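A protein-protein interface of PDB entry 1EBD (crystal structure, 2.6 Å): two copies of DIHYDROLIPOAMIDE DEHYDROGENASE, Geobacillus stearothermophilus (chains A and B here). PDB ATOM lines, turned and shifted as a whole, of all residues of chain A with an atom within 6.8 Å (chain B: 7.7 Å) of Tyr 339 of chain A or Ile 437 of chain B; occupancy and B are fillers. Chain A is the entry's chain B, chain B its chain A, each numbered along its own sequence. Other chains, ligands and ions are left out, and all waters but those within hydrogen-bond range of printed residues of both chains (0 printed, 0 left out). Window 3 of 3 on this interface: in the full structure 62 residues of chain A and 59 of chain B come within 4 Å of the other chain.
Of the printed residues of chain B, Tyr 339 of chain A touches Ile 437. Printed residues of chain A within 4 Å of Ile 437 of chain B: His 317 (3.6 Å), Tyr 321 (3.7 Å), Tyr 339 (3.98 Å), Ile 342 (3.6 Å) and Pro 343 (3.1 Å). Printed residues of chain A within 4 Å of Glu 445 of chain B: His 317. Of the printed residues of chain A, Ala 439 of chain B touches His 317. Of the printed residues of chain A, His 438 of chain B touches His 317 (2.4 Å). The nearest printed residue of chain A that does not touch Ile 437 of chain B is Ala 341 of chain A (4.7 Å). The nearest printed residue of chain A that does not touch His 438 of chain B is Pro 343 of chain A (4.4 Å).
Printed residues of chain B that touch a printed residue of chain A: Thr 436, Ile 437, His 438, Ala 439, His 440, Glu 445 and Met 448. Hydrophobic or aromatic side chains of chain B that line the printed part of chain A: Ile 437, His 440 and Met 448. Among the printed residues, no Asp or Glu carboxylate lies within 4 Å of a Lys or Arg side-chain nitrogen of the other chain.
Among the printed residues, merely in contact across the chains: Pro 343 of chain A with Ile 437 of chain B (3.1 Å), His 317 of chain A with His 440 of chain B (3.5 Å), His 317 of chain A with Ile 437 of chain B (3.6 Å), Leu 422 of chain A with Thr 436 of chain B (3.6 Å), Glu 425 of chain A with Thr 436 of chain B (3.6 Å), Ile 342 of chain A with Ile 437 of chain B (3.6 Å), Tyr 321 of chain A with Ile 437 of chain B (3.7 Å), His 317 of chain A with Ala 439 of chain B (3.7 Å), His 317 of chain A with Met 448 of chain B (3.8 Å) and Tyr 339 of chain A with Ile 437 of chain B (3.98 Å).
No position is printed for both chains.
The side-chain carboxylate (OE2) of Glu 445 of chain B is in hydrogen-bond range of a ring nitrogen (ND1) of His 440 of chain B, 2.5 Å away. OH of Tyr 321 of chain A sits at hydrogen-bond distance from N of Asp 338 of chain A. The side-chain hydroxyl (OG1) of Thr 436 of chain B is in hydrogen-bond range of the backbone carbonyl oxygen (O) of Asp 432 of chain B (2.9 Å). N of Ala 341 of chain A sits at hydrogen-bond distance from OE1 of Glu 425 of chain A, at 3.4 Å. The side-chain carboxylate (OE2) of Glu 425 of chain A sits at hydrogen-bond distance from the backbone NH (N) of Val 340 of chain A, at 2.8 Å.
The side-chain carboxylate of Glu 445 of chain B sits at hydrogen-bond distance from a ring nitrogen (NE2) of His 317 of chain A (2.6 Å). O of His 438 of chain B sits at hydrogen-bond distance from ND1 of His 317 of chain A.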
ATOM      1  N   PRO A 311      13.466  13.677  41.292  1.00  0.00           N
ATOM      2  CA  PRO A 311      13.742  12.240  41.177  1.00  0.00           C
ATOM      3  C   PRO A 311      13.969  11.736  39.756  1.00  0.00           C
ATOM      4  O   PRO A 311      13.577  12.385  38.782  1.00  0.00           O
ATOM      5  CB  PRO A 311      12.502  11.608  41.807  1.00  0.00           C
ATOM      6  CG  PRO A 311      12.071  12.647  42.809  1.00  0.00           C
ATOM      7  CD  PRO A 311      12.194  13.904  41.996  1.00  0.00           C
ATOM      8  N   GLY A 312      14.568  10.550  39.653  1.00  0.00           N
ATOM      9  CA  GLY A 312      14.847   9.953  38.357  1.00  0.00           C
ATOM     10  C   GLY A 312      16.342   9.829  38.114  1.00  0.00           C
ATOM     11  O   GLY A 312      17.124  10.122  39.020  1.00  0.00           O
ATOM     12  N   PRO A 313      16.773   9.382  36.917  1.00  0.00           N
ATOM     13  CA  PRO A 313      18.188   9.219  36.563  1.00  0.00           C
ATOM     14  C   PRO A 313      18.894  10.561  36.381  1.00  0.00           C
ATOM     15  O   PRO A 313      18.414  11.428  35.654  1.00  0.00           O
ATOM     16  CB  PRO A 313      18.122   8.462  35.235  1.00  0.00           C
ATOM     17  CG  PRO A 313      16.785   7.799  35.264  1.00  0.00           C
ATOM     18  CD  PRO A 313      15.925   8.881  35.827  1.00  0.00           C
ATOM     19  N   HIS A 317      19.753  14.331  29.526  1.00  0.00           N
ATOM     20  CA  HIS A 317      18.555  14.170  28.701  1.00  0.00           C
ATOM     21  C   HIS A 317      17.261  14.124  29.495  1.00  0.00           C
ATOM     22  O   HIS A 317      16.219  14.575  29.019  1.00  0.00           O
ATOM     23  CB  HIS A 317      18.673  12.946  27.789  1.00  0.00           C
ATOM     24  CG  HIS A 317      19.111  13.274  26.391  1.00  0.00           C
ATOM     25  ND1 HIS A 317      18.770  12.501  25.303  1.00  0.00           N
ATOM     26  CD2 HIS A 317      19.855  14.297  25.901  1.00  0.00           C
ATOM     27  CE1 HIS A 317      19.283  13.027  24.206  1.00  0.00           C
ATOM     28  NE2 HIS A 317      19.944  14.121  24.540  1.00  0.00           N
ATOM     29  N   LYS A 318      17.322  13.573  30.701  1.00  0.00           N
ATOM     30  CA  LYS A 318      16.149  13.506  31.563  1.00  0.00           C
ATOM     31  C   LYS A 318      15.846  14.954  31.928  1.00  0.00           C
ATOM     32  O   LYS A 318      14.690  15.346  32.018  1.00  0.00           O
ATOM     33  CB  LYS A 318      16.448  12.681  32.821  1.00  0.00           C
ATOM     34  CG  LYS A 318      15.216  12.222  33.599  1.00  0.00           C
ATOM     35  CD  LYS A 318      14.846  13.168  34.723  1.00  0.00           C
ATOM     36  CE  LYS A 318      15.831  13.076  35.876  1.00  0.00           C
ATOM     37  NZ  LYS A 318      15.502  14.002  36.995  1.00  0.00           N
ATOM     38  N   TYR A 321      14.405  16.903  28.681  1.00  0.00           N
ATOM     39  CA  TYR A 321      13.044  16.457  28.419  1.00  0.00           C
ATOM     40  C   TYR A 321      12.065  17.180  29.334  1.00  0.00           C
ATOM     41  O   TYR A 321      11.078  17.765  28.880  1.00  0.00           O
ATOM     42  CB  TYR A 321      12.967  14.957  28.651  1.00  0.00           C
ATOM     43  CG  TYR A 321      11.603  14.349  28.484  1.00  0.00           C
ATOM     44  CD1 TYR A 321      11.128  13.987  27.226  1.00  0.00           C
ATOM     45  CD2 TYR A 321      10.824  14.048  29.591  1.00  0.00           C
ATOM     46  CE1 TYR A 321       9.912  13.328  27.081  1.00  0.00           C
ATOM     47  CE2 TYR A 321       9.613  13.393  29.460  1.00  0.00           C
ATOM     48  CZ  TYR A 321       9.165  13.030  28.209  1.00  0.00           C
ATOM     49  OH  TYR A 321       7.991  12.324  28.108  1.00  0.00           O
ATOM     50  N   GLU A 322      12.348  17.141  30.629  1.00  0.00           N
ATOM     51  CA  GLU A 322      11.501  17.801  31.601  1.00  0.00           C
ATOM     52  C   GLU A 322      11.465  19.291  31.300  1.00  0.00           C
ATOM     53  O   GLU A 322      10.421  19.920  31.414  1.00  0.00           O
ATOM     54  CB  GLU A 322      12.029  17.555  33.005  1.00  0.00           C
ATOM     55  CG  GLU A 322      12.034  16.091  33.383  1.00  0.00           C
ATOM     56  CD  GLU A 322      12.655  15.834  34.743  1.00  0.00           C
ATOM     57  OE1 GLU A 322      13.548  16.605  35.161  1.00  0.00           O
ATOM     58  OE2 GLU A 322      12.254  14.844  35.394  1.00  0.00           O
ATOM     59  N   ALA A 336       3.010  16.382  29.805  1.00  0.00           N
ATOM     60  CA  ALA A 336       3.219  15.517  30.956  1.00  0.00           C
ATOM     61  C   ALA A 336       4.486  14.717  30.708  1.00  0.00           C
ATOM     62  O   ALA A 336       4.975  14.666  29.581  1.00  0.00           O
ATOM     63  CB  ALA A 336       2.029  14.583  31.142  1.00  0.00           C
ATOM     64  N   VAL A 337       5.045  14.135  31.760  1.00  0.00           N
ATOM     65  CA  VAL A 337       6.254  13.336  31.626  1.00  0.00           C
ATOM     66  C   VAL A 337       5.820  11.932  31.241  1.00  0.00           C
ATOM     67  O   VAL A 337       5.198  11.224  32.032  1.00  0.00           O
ATOM     68  CB  VAL A 337       7.082  13.321  32.942  1.00  0.00           C
ATOM     69  CG1 VAL A 337       8.255  12.359  32.828  1.00  0.00           C
ATOM     70  CG2 VAL A 337       7.599  14.725  33.250  1.00  0.00           C
ATOM     71  N   ASP A 338       6.110  11.550  30.004  1.00  0.00           N
ATOM     72  CA  ASP A 338       5.727  10.236  29.512  1.00  0.00           C
ATOM     73  C   ASP A 338       6.797   9.534  28.667  1.00  0.00           C
ATOM     74  O   ASP A 338       6.941   9.781  27.470  1.00  0.00           O
ATOM     75  CB  ASP A 338       4.417  10.361  28.722  1.00  0.00           C
ATOM     76  CG  ASP A 338       3.788   9.017  28.388  1.00  0.00           C
ATOM     77  OD1 ASP A 338       4.240   7.969  28.914  1.00  0.00           O
ATOM     78  OD2 ASP A 338       2.822   9.017  27.594  1.00  0.00           O
ATOM     79  N   TYR A 339       7.564   8.669  29.309  1.00  0.00           N
ATOM     80  CA  TYR A 339       8.581   7.911  28.616  1.00  0.00           C
ATOM     81  C   TYR A 339       8.633   6.568  29.297  1.00  0.00           C
ATOM     82  O   TYR A 339       8.369   6.474  30.489  1.00  0.00           O
ATOM     83  CB  TYR A 339       9.943   8.611  28.647  1.00  0.00           C
ATOM     84  CG  TYR A 339      10.486   8.985  30.008  1.00  0.00           C
ATOM     85  CD1 TYR A 339      11.168   8.057  30.793  1.00  0.00           C
ATOM     86  CD2 TYR A 339      10.382  10.292  30.480  1.00  0.00           C
ATOM     87  CE1 TYR A 339      11.736   8.424  32.014  1.00  0.00           C
ATOM     88  CE2 TYR A 339      10.952  10.667  31.696  1.00  0.00           C
ATOM     89  CZ  TYR A 339      11.627   9.729  32.455  1.00  0.00           C
ATOM     90  OH  TYR A 339      12.208  10.101  33.647  1.00  0.00           O
ATOM     91  N   VAL A 340       8.909   5.515  28.543  1.00  0.00           N
ATOM     92  CA  VAL A 340       8.944   4.192  29.137  1.00  0.00           C
ATOM     93  C   VAL A 340      10.336   3.831  29.614  1.00  0.00           C
ATOM     94  O   VAL A 340      10.505   2.866  30.356  1.00  0.00           O
ATOM     95  CB  VAL A 340       8.372   3.094  28.181  1.00  0.00           C
ATOM     96  CG1 VAL A 340       7.659   3.732  26.998  1.00  0.00           C
ATOM     97  CG2 VAL A 340       9.446   2.136  27.710  1.00  0.00           C
ATOM     98  N   ALA A 341      11.331   4.609  29.196  1.00  0.00           N
ATOM     99  CA  ALA A 341      12.713   4.348  29.587  1.00  0.00           C
ATOM    100  C   ALA A 341      13.662   5.399  29.058  1.00  0.00           C
ATOM    101  O   ALA A 341      13.315   6.166  28.162  1.00  0.00           O
ATOM    102  CB  ALA A 341      13.159   2.976  29.088  1.00  0.00           C
ATOM    103  N   ILE A 342      14.847   5.442  29.655  1.00  0.00           N
ATOM    104  CA  ILE A 342      15.901   6.357  29.249  1.00  0.00           C
ATOM    105  C   ILE A 342      17.155   5.506  29.218  1.00  0.00           C
ATOM    106  O   ILE A 342      17.347   4.653  30.085  1.00  0.00           O
ATOM    107  CB  ILE A 342      16.102   7.521  30.239  1.00  0.00           C
ATOM    108  CG1 ILE A 342      14.860   8.402  30.266  1.00  0.00           C
ATOM    109  CG2 ILE A 342      17.287   8.384  29.810  1.00  0.00           C
ATOM    110  CD1 ILE A 342      15.087   9.725  30.947  1.00  0.00           C
ATOM    111  N   PRO A 343      17.947   5.629  28.142  1.00  0.00           N
ATOM    112  CA  PRO A 343      19.192   4.877  27.976  1.00  0.00           C
ATOM    113  C   PRO A 343      20.318   5.525  28.770  1.00  0.00           C
ATOM    114  O   PRO A 343      20.404   6.755  28.863  1.00  0.00           O
ATOM    115  CB  PRO A 343      19.463   4.991  26.475  1.00  0.00           C
ATOM    116  CG  PRO A 343      18.121   5.361  25.880  1.00  0.00           C
ATOM    117  CD  PRO A 343      17.587   6.308  26.892  1.00  0.00           C
ATOM    118  N   VAL A 355      19.153   0.168  28.865  1.00  0.00           N
ATOM    119  CA  VAL A 355      17.859   0.824  28.747  1.00  0.00           C
ATOM    120  C   VAL A 355      16.794  -0.195  29.148  1.00  0.00           C
ATOM    121  O   VAL A 355      16.923  -1.392  28.862  1.00  0.00           O
ATOM    122  CB  VAL A 355      17.616   1.341  27.311  1.00  0.00           C
ATOM    123  CG1 VAL A 355      17.475   0.186  26.336  1.00  0.00           C
ATOM    124  CG2 VAL A 355      16.401   2.246  27.277  1.00  0.00           C
ATOM    125  N   GLY A 421      16.317   1.129  22.142  1.00  0.00           N
ATOM    126  CA  GLY A 421      15.589   2.131  22.899  1.00  0.00           C
ATOM    127  C   GLY A 421      14.279   2.515  22.232  1.00  0.00           C
ATOM    128  O   GLY A 421      13.229   2.511  22.876  1.00  0.00           O
ATOM    129  N   LEU A 422      14.339   2.837  20.942  1.00  0.00           N
ATOM    130  CA  LEU A 422      13.157   3.218  20.175  1.00  0.00           C
ATOM    131  C   LEU A 422      12.145   2.082  20.220  1.00  0.00           C
ATOM    132  O   LEU A 422      10.939   2.318  20.275  1.00  0.00           O
ATOM    133  CB  LEU A 422      13.530   3.506  18.719  1.00  0.00           C
ATOM    134  CG  LEU A 422      12.428   4.063  17.811  1.00  0.00           C
ATOM    135  CD1 LEU A 422      12.225   5.553  18.078  1.00  0.00           C
ATOM    136  CD2 LEU A 422      12.805   3.848  16.357  1.00  0.00           C
ATOM    137  N   GLU A 425      10.435   2.063  23.861  1.00  0.00           N
ATOM    138  CA  GLU A 425       9.548   3.209  23.924  1.00  0.00           C
ATOM    139  C   GLU A 425       8.241   3.031  23.144  1.00  0.00           C
ATOM    140  O   GLU A 425       7.191   3.503  23.574  1.00  0.00           O
ATOM    141  CB  GLU A 425      10.293   4.445  23.421  1.00  0.00           C
ATOM    142  CG  GLU A 425       9.689   5.762  23.848  1.00  0.00           C
ATOM    143  CD  GLU A 425       9.732   5.980  25.350  1.00  0.00           C
ATOM    144  OE1 GLU A 425      10.762   5.662  25.989  1.00  0.00           O
ATOM    145  OE2 GLU A 425       8.729   6.489  25.889  1.00  0.00           O
ATOM    146  N   ASP B 432       7.413  10.269  16.589  1.00  0.00           N
ATOM    147  CA  ASP B 432       7.681   9.082  17.394  1.00  0.00           C
ATOM    148  C   ASP B 432       9.135   9.027  17.804  1.00  0.00           C
ATOM    149  O   ASP B 432       9.457   8.586  18.906  1.00  0.00           O
ATOM    150  CB  ASP B 432       7.337   7.810  16.629  1.00  0.00           C
ATOM    151  CG  ASP B 432       5.919   7.363  16.868  1.00  0.00           C
ATOM    152  OD1 ASP B 432       5.480   7.402  18.034  1.00  0.00           O
ATOM    153  OD2 ASP B 432       5.238   6.973  15.897  1.00  0.00           O
ATOM    154  N   ILE B 433      10.008   9.464  16.901  1.00  0.00           N
ATOM    155  CA  ILE B 433      11.438   9.487  17.166  1.00  0.00           C
ATOM    156  C   ILE B 433      11.788  10.672  18.073  1.00  0.00           C
ATOM    157  O   ILE B 433      12.550  10.516  19.022  1.00  0.00           O
ATOM    158  CB  ILE B 433      12.279   9.575  15.852  1.00  0.00           C
ATOM    159  CG1 ILE B 433      12.121   8.299  15.025  1.00  0.00           C
ATOM    160  CG2 ILE B 433      13.758   9.771  16.171  1.00  0.00           C
ATOM    161  CD1 ILE B 433      13.075   8.221  13.835  1.00  0.00           C
ATOM    162  N   ALA B 434      11.208  11.840  17.794  1.00  0.00           N
ATOM    163  CA  ALA B 434      11.483  13.052  18.567  1.00  0.00           C
ATOM    164  C   ALA B 434      11.053  12.966  20.021  1.00  0.00           C
ATOM    165  O   ALA B 434      11.623  13.634  20.884  1.00  0.00           O
ATOM    166  CB  ALA B 434      10.843  14.250  17.912  1.00  0.00           C
ATOM    167  N   LEU B 435      10.030  12.165  20.292  1.00  0.00           N
ATOM    168  CA  LEU B 435       9.558  12.018  21.655  1.00  0.00           C
ATOM    169  C   LEU B 435      10.410  11.028  22.441  1.00  0.00           C
ATOM    170  O   LEU B 435      10.443  11.068  23.669  1.00  0.00           O
ATOM    171  CB  LEU B 435       8.091  11.605  21.670  1.00  0.00           C
ATOM    172  CG  LEU B 435       7.113  12.533  20.938  1.00  0.00           C
ATOM    173  CD1 LEU B 435       5.715  12.295  21.479  1.00  0.00           C
ATOM    174  CD2 LEU B 435       7.488  14.000  21.113  1.00  0.00           C
ATOM    175  N   THR B 436      11.099  10.141  21.729  1.00  0.00           N
ATOM    176  CA  THR B 436      11.968   9.140  22.352  1.00  0.00           C
ATOM    177  C   THR B 436      13.286   9.757  22.861  1.00  0.00           C
ATOM    178  O   THR B 436      13.983  10.465  22.128  1.00  0.00           O
ATOM    179  CB  THR B 436      12.286   8.004  21.355  1.00  0.00           C
ATOM    180  OG1 THR B 436      11.066   7.371  20.948  1.00  0.00           O
ATOM    181  CG2 THR B 436      13.200   6.970  21.980  1.00  0.00           C
ATOM    182  N   ILE B 437      13.636   9.471  24.112  1.00  0.00           N
ATOM    183  CA  ILE B 437      14.863  10.004  24.683  1.00  0.00           C
ATOM    184  C   ILE B 437      16.042   9.129  24.316  1.00  0.00           C
ATOM    185  O   ILE B 437      16.100   7.957  24.683  1.00  0.00           O
ATOM    186  CB  ILE B 437      14.783  10.128  26.207  1.00  0.00           C
ATOM    187  CG1 ILE B 437      13.659  11.095  26.592  1.00  0.00           C
ATOM    188  CG2 ILE B 437      16.110  10.632  26.757  1.00  0.00           C
ATOM    189  CD1 ILE B 437      13.428  11.207  28.084  1.00  0.00           C
ATOM    190  N   HIS B 438      16.947   9.693  23.526  1.00  0.00           N
ATOM    191  CA  HIS B 438      18.147   8.985  23.091  1.00  0.00           C
ATOM    192  C   HIS B 438      19.252   9.229  24.112  1.00  0.00           C
ATOM    193  O   HIS B 438      19.155  10.153  24.916  1.00  0.00           O
ATOM    194  CB  HIS B 438      18.585   9.495  21.719  1.00  0.00           C
ATOM    195  CG  HIS B 438      17.588   9.243  20.637  1.00  0.00           C
ATOM    196  ND1 HIS B 438      17.950   8.845  19.370  1.00  0.00           N
ATOM    197  CD2 HIS B 438      16.235   9.320  20.636  1.00  0.00           C
ATOM    198  CE1 HIS B 438      16.864   8.686  18.635  1.00  0.00           C
ATOM    199  NE2 HIS B 438      15.811   8.966  19.379  1.00  0.00           N
ATOM    200  N   ALA B 439      20.307   8.426  24.076  1.00  0.00           N
ATOM    201  CA  ALA B 439      21.408   8.593  25.012  1.00  0.00           C
ATOM    202  C   ALA B 439      22.145   9.917  24.785  1.00  0.00           C
ATOM    203  O   ALA B 439      21.964  10.576  23.755  1.00  0.00           O
ATOM    204  CB  ALA B 439      22.363   7.423  24.894  1.00  0.00           C
ATOM    205  N   HIS B 440      22.946  10.322  25.765  1.00  0.00           N
ATOM    206  CA  HIS B 440      23.712  11.564  25.680  1.00  0.00           C
ATOM    207  C   HIS B 440      25.028  11.423  26.432  1.00  0.00           C
ATOM    208  O   HIS B 440      25.072  10.837  27.519  1.00  0.00           O
ATOM    209  CB  HIS B 440      22.906  12.714  26.277  1.00  0.00           C
ATOM    210  CG  HIS B 440      23.635  14.026  26.309  1.00  0.00           C
ATOM    211  ND1 HIS B 440      23.217  15.126  25.594  1.00  0.00           N
ATOM    212  CD2 HIS B 440      24.739  14.419  26.989  1.00  0.00           C
ATOM    213  CE1 HIS B 440      24.031  16.138  25.825  1.00  0.00           C
ATOM    214  NE2 HIS B 440      24.964  15.735  26.671  1.00  0.00           N
ATOM    215  N   GLU B 445      21.954  10.528  19.276  1.00  0.00           N
ATOM    216  CA  GLU B 445      21.192  11.679  19.759  1.00  0.00           C
ATOM    217  C   GLU B 445      20.759  12.489  18.521  1.00  0.00           C
ATOM    218  O   GLU B 445      19.643  13.004  18.467  1.00  0.00           O
ATOM    219  CB  GLU B 445      22.090  12.517  20.722  1.00  0.00           C
ATOM    220  CG  GLU B 445      21.423  13.662  21.563  1.00  0.00           C
ATOM    221  CD  GLU B 445      22.376  14.286  22.622  1.00  0.00           C
ATOM    222  OE1 GLU B 445      23.526  13.787  22.692  1.00  0.00           O
ATOM    223  OE2 GLU B 445      21.989  15.255  23.371  1.00  0.00           O
ATOM    224  N   MET B 448      17.295  11.980  16.940  1.00  0.00           N
ATOM    225  CA  MET B 448      16.240  12.630  17.707  1.00  0.00           C
ATOM    226  C   MET B 448      16.193  14.112  17.342  1.00  0.00           C
ATOM    227  O   MET B 448      15.125  14.647  17.036  1.00  0.00           O
ATOM    228  CB  MET B 448      16.506  12.466  19.200  1.00  0.00           C
ATOM    229  CG  MET B 448      15.384  12.939  20.103  1.00  0.00           C
ATOM    230  SD  MET B 448      15.920  12.940  21.829  1.00  0.00           S
ATOM    231  CE  MET B 448      16.721  14.457  21.852  1.00  0.00           C
